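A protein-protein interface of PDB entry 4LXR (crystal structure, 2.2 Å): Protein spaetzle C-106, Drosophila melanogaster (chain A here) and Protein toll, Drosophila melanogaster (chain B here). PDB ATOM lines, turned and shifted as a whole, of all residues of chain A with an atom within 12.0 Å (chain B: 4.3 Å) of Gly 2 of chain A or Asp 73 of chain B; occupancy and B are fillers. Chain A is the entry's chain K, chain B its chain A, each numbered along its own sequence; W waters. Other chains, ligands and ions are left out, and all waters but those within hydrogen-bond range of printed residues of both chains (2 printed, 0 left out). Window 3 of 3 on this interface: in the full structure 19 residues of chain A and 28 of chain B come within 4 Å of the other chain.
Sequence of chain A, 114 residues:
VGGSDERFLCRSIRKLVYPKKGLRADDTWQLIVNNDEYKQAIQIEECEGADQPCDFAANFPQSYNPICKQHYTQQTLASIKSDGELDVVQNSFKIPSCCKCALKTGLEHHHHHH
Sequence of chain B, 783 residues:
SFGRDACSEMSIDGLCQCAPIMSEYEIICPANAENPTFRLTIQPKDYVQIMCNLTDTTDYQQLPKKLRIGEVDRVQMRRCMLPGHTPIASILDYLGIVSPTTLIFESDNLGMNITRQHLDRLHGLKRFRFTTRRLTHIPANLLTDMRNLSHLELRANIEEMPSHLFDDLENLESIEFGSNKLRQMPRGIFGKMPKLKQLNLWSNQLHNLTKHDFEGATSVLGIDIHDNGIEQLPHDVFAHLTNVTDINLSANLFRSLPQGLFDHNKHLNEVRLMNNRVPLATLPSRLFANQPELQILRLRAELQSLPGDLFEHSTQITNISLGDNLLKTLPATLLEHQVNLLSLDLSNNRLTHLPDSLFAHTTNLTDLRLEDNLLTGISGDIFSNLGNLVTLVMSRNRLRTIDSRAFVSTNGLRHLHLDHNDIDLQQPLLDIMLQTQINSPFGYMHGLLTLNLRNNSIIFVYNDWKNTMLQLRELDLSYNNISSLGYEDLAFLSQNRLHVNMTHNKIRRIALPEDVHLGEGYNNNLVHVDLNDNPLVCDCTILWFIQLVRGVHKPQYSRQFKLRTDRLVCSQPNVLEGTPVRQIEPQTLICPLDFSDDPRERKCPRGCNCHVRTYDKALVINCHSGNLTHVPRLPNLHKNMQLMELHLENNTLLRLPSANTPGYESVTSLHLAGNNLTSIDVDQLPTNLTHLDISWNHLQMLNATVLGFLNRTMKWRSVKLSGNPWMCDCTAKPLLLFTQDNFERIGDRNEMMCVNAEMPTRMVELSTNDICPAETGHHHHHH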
ATOM      1  N   VAL A   1     -31.592 -19.458  15.637  1.00  0.00           N
ATOM      2  CA  VAL A   1     -30.772 -18.908  14.561  1.00  0.00           C
ATOM      3  C   VAL A   1     -29.663 -19.900  14.195  1.00  0.00           C
ATOM      4  O   VAL A   1     -29.709 -21.072  14.596  1.00  0.00           O
ATOM      5  CB  VAL A   1     -30.148 -17.565  14.983  1.00  0.00           C
ATOM      6  CG1 VAL A   1     -30.084 -16.599  13.796  1.00  0.00           C
ATOM      7  CG2 VAL A   1     -30.946 -16.956  16.134  1.00  0.00           C
ATOM      8  N   GLY A   2     -28.670 -19.435  13.440  1.00  0.00           N
ATOM      9  CA  GLY A   2     -27.524 -20.269  13.114  1.00  0.00           C
ATOM     10  C   GLY A   2     -26.597 -20.551  14.291  1.00  0.00           C
ATOM     11  O   GLY A   2     -26.516 -19.763  15.234  1.00  0.00           O
ATOM     12  N   GLY A   3     -25.902 -21.686  14.237  1.00  0.00           N
ATOM     13  CA  GLY A   3     -24.897 -22.030  15.234  1.00  0.00           C
ATOM     14  C   GLY A   3     -25.370 -22.877  16.407  1.00  0.00           C
ATOM     15  O   GLY A   3     -24.595 -23.185  17.309  1.00  0.00           O
ATOM     16  N   SER A   4     -26.642 -23.251  16.418  1.00  0.00           N
ATOM     17  CA  SER A   4     -27.154 -24.095  17.497  1.00  0.00           C
ATOM     18  C   SER A   4     -26.999 -25.574  17.151  1.00  0.00           C
ATOM     19  O   SER A   4     -26.823 -25.941  15.989  1.00  0.00           O
ATOM     20  CB  SER A   4     -28.618 -23.770  17.805  1.00  0.00           C
ATOM     21  OG  SER A   4     -29.456 -24.202  16.747  1.00  0.00           O
ATOM     22  N   ASP A   5     -27.073 -26.422  18.164  1.00  0.00           N
ATOM     23  CA  ASP A   5     -26.858 -27.843  17.979  1.00  0.00           C
ATOM     24  C   ASP A   5     -27.395 -28.546  19.211  1.00  0.00           C
ATOM     25  O   ASP A   5     -27.100 -28.152  20.331  1.00  0.00           O
ATOM     26  CB  ASP A   5     -25.363 -28.114  17.846  1.00  0.00           C
ATOM     27  CG  ASP A   5     -25.047 -29.549  17.469  1.00  0.00           C
ATOM     28  OD1 ASP A   5     -25.804 -30.175  16.687  1.00  0.00           O
ATOM     29  OD2 ASP A   5     -24.013 -30.042  17.942  1.00  0.00           O
ATOM     30  N   GLU A   6     -28.189 -29.583  19.012  1.00  0.00           N
ATOM     31  CA  GLU A   6     -28.707 -30.356  20.132  1.00  0.00           C
ATOM     32  C   GLU A   6     -27.767 -31.510  20.408  1.00  0.00           C
ATOM     33  O   GLU A   6     -27.323 -32.188  19.495  1.00  0.00           O
ATOM     34  CB  GLU A   6     -30.089 -30.906  19.803  1.00  0.00           C
ATOM     35  CG  GLU A   6     -31.132 -29.854  19.601  1.00  0.00           C
ATOM     36  CD  GLU A   6     -32.517 -30.457  19.461  1.00  0.00           C
ATOM     37  OE1 GLU A   6     -32.608 -31.620  19.011  1.00  0.00           O
ATOM     38  OE2 GLU A   6     -33.504 -29.777  19.815  1.00  0.00           O
ATOM     39  N   LYS B  45     -31.163 -26.033   3.818  1.00  0.00           N
ATOM     40  CA  LYS B  45     -30.880 -24.774   4.523  1.00  0.00           C
ATOM     41  C   LYS B  45     -30.490 -24.965   5.983  1.00  0.00           C
ATOM     42  O   LYS B  45     -29.874 -24.081   6.578  1.00  0.00           O
ATOM     43  CB  LYS B  45     -32.040 -23.770   4.431  1.00  0.00           C
ATOM     44  CG  LYS B  45     -32.379 -23.310   3.026  1.00  0.00           C
ATOM     45  CD  LYS B  45     -33.500 -22.276   3.047  1.00  0.00           C
ATOM     46  CE  LYS B  45     -34.000 -21.957   1.638  1.00  0.00           C
ATOM     47  NZ  LYS B  45     -35.224 -21.099   1.633  1.00  0.00           N
ATOM     48  N   ASP B  46     -30.845 -26.110   6.560  1.00  0.00           N
ATOM     49  CA  ASP B  46     -30.604 -26.343   7.983  1.00  0.00           C
ATOM     50  C   ASP B  46     -29.298 -27.100   8.232  1.00  0.00           C
ATOM     51  O   ASP B  46     -28.341 -26.558   8.795  1.00  0.00           O
ATOM     52  CB  ASP B  46     -31.792 -27.075   8.620  1.00  0.00           C
ATOM     53  CG  ASP B  46     -31.690 -27.162  10.138  1.00  0.00           C
ATOM     54  OD1 ASP B  46     -30.871 -26.433  10.735  1.00  0.00           O
ATOM     55  OD2 ASP B  46     -32.448 -27.955  10.741  1.00  0.00           O
ATOM     56  N   VAL B  72     -26.216 -23.987   3.757  1.00  0.00           N
ATOM     57  CA  VAL B  72     -26.657 -24.820   4.860  1.00  0.00           C
ATOM     58  C   VAL B  72     -25.939 -24.395   6.148  1.00  0.00           C
ATOM     59  O   VAL B  72     -24.771 -24.019   6.111  1.00  0.00           O
ATOM     60  CB  VAL B  72     -26.464 -26.317   4.508  1.00  0.00           C
ATOM     61  CG1 VAL B  72     -24.994 -26.749   4.662  1.00  0.00           C
ATOM     62  CG2 VAL B  72     -27.380 -27.168   5.329  1.00  0.00           C
ATOM     63  N   ASP B  73     -26.648 -24.417   7.275  1.00  0.00           N
ATOM     64  CA  ASP B  73     -26.123 -23.874   8.535  1.00  0.00           C
ATOM     65  C   ASP B  73     -25.067 -24.765   9.196  1.00  0.00           C
ATOM     66  O   ASP B  73     -24.004 -24.300   9.624  1.00  0.00           O
ATOM     67  CB  ASP B  73     -27.283 -23.586   9.508  1.00  0.00           C
ATOM     68  CG  ASP B  73     -26.823 -23.400  10.956  1.00  0.00           C
ATOM     69  OD1 ASP B  73     -26.157 -22.390  11.266  1.00  0.00           O
ATOM     70  OD2 ASP B  73     -27.159 -24.259  11.797  1.00  0.00           O
ATOM     71  N   ARG B  74     -25.364 -26.053   9.251  1.00  0.00           N
ATOM     72  CA  ARG B  74     -24.561 -26.998   9.992  1.00  0.00           C
ATOM     73  C   ARG B  74     -24.141 -28.178   9.104  1.00  0.00           C
ATOM     74  O   ARG B  74     -24.971 -28.777   8.414  1.00  0.00           O
ATOM     75  CB  ARG B  74     -25.360 -27.482  11.210  1.00  0.00           C
ATOM     76  CG  ARG B  74     -24.587 -28.397  12.141  1.00  0.00           C
ATOM     77  CD  ARG B  74     -25.358 -28.696  13.426  1.00  0.00           C
ATOM     78  NE  ARG B  74     -26.376 -29.723  13.226  1.00  0.00           N
ATOM     79  CZ  ARG B  74     -27.683 -29.507  13.306  1.00  0.00           C
ATOM     80  NH1 ARG B  74     -28.534 -30.508  13.104  1.00  0.00           N
ATOM     81  NH2 ARG B  74     -28.141 -28.290  13.599  1.00  0.00           N
ATOM     82  N   PRO B 100     -21.118 -22.879   5.257  1.00  0.00           N
ATOM     83  CA  PRO B 100     -21.664 -23.393   6.511  1.00  0.00           C
ATOM     84  C   PRO B 100     -21.210 -22.514   7.672  1.00  0.00           C
ATOM     85  O   PRO B 100     -20.193 -21.849   7.562  1.00  0.00           O
ATOM     86  CB  PRO B 100     -21.010 -24.769   6.619  1.00  0.00           C
ATOM     87  CG  PRO B 100     -19.693 -24.584   5.951  1.00  0.00           C
ATOM     88  CD  PRO B 100     -20.004 -23.703   4.766  1.00  0.00           C
ATOM     89  N   THR B 101     -21.959 -22.535   8.765  1.00  0.00           N
ATOM     90  CA  THR B 101     -21.666 -21.769   9.970  1.00  0.00           C
ATOM     91  C   THR B 101     -20.949 -22.672  10.987  1.00  0.00           C
ATOM     92  O   THR B 101     -20.160 -22.227  11.837  1.00  0.00           O
ATOM     93  CB  THR B 101     -23.013 -21.267  10.566  1.00  0.00           C
ATOM     94  OG1 THR B 101     -23.368 -20.024   9.954  1.00  0.00           O
ATOM     95  CG2 THR B 101     -22.954 -21.081  12.083  1.00  0.00           C
ATOM     96  N   THR B 102     -21.250 -23.960  10.883  1.00  0.00           N
ATOM     97  CA  THR B 102     -20.874 -24.941  11.879  1.00  0.00           C
ATOM     98  C   THR B 102     -20.343 -26.166  11.161  1.00  0.00           C
ATOM     99  O   THR B 102     -20.974 -26.671  10.233  1.00  0.00           O
ATOM    100  CB  THR B 102     -22.099 -25.336  12.735  1.00  0.00           C
ATOM    101  OG1 THR B 102     -22.488 -24.220  13.536  1.00  0.00           O
ATOM    102  CG2 THR B 102     -21.810 -26.519  13.652  1.00  0.00           C
HETATM  103  O   HOH W   1     -28.676 -23.416  14.285  1.00  0.00           O
HETATM  104  O   HOH W   2     -25.269 -25.161  13.898  1.00  0.00           O
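The side-chain carboxylate (OD1) of Asp 73 of chain B lies within hydrogen-bond range of the backbone NH (N) of Gly 3 of chain A, 3.1 Å away.
The side-chain carboxylate (OD1) of Asp 5 of chain A is in salt-bridge range of the guanidinium group (NE) of Arg 74 of chain B (3.5 Å).
The backbone carbonyl oxygen (O) of Lys 45 of chain B sits at hydrogen-bond distance from the backbone NH (N) of Asp 73 of chain B (3.3 Å).
The backbone NH (N) of Asp 73 of chain B lies within hydrogen-bond range of the backbone carbonyl oxygen (O) of Asp 46 of chain B (3.1 Å).
The backbone NH (N) of Arg 74 of chain B lies within hydrogen-bond range of the backbone carbonyl oxygen (O) of Asp 46 of chain B.
The backbone carbonyl oxygen (O) of Asp 73 of chain B is in hydrogen-bond range of the backbone NH (N) of Thr 101 of chain B (2.8 Å).
O of Asp 73 of chain B lies within hydrogen-bond range of N of Thr 102 of chain B (3.0 Å).
Gly 2 of chain A touches Asp 73 of chain B.
Gly 3 of chain A touches Thr 101 of chain B (N to CG2, 3.7 Å).
Thr 102 of chain B touches Gly 3 of chain A.
Ser 4 of chain A touches Arg 74 of chain B (O to NH2, 3.6 Å).
Gly 2 of chain A touches just one residue of chain B: Asp 73 (3.1 Å).
Of the printed residues of chain B, Gly 3 of chain A touches Asp 73, Thr 101 and Thr 102.
Of the printed residues of chain B, Ser 4 of chain A touches Arg 74.
Asp 46 of chain B touches none of the printed residues of chain A.
No residue of chain A comes within 4 Å of Val 72 of chain B.
Asp 73 of chain B touches just these residues of chain A: Gly 2 and Gly 3.
Printed residues of chain A within 4 Å of Arg 74 of chain B: Ser 4 (3.6 Å) and Asp 5 (3.5 Å).
Of the printed residues of chain A, Thr 102 of chain B touches Gly 3.
The nearest printed residue of chain B that does not touch Gly 2 of chain A is Thr 101 of chain B (4.3 Å).
The nearest printed residue of chain B that does not touch Gly 3 of chain A is Arg 74 of chain B (6.5 Å).
Among the printed residues, 6 pairs touch across the chains.
Among the printed residues, Asp or Glu carboxylates within 4 Å of a Lys or Arg side-chain nitrogen of the other chain: Asp 5 of chain A with Arg 74 of chain B (3.5 Å).
Water W1 lies within hydrogen-bond range of the backbone carbonyl oxygen (O) of Val 1 of chain A, the side-chain hydroxyl (OG) of Ser 4 of chain A, the side-chain carboxylate (OD2) of Asp 73 of chain B and the backbone NH (N) of Gly 3 of chain A.
Water W2 lies within hydrogen-bond range of O of Ser 4 of chain A, OG1 of Thr 102 of chain B and OD2 of Asp 73 of chain B.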
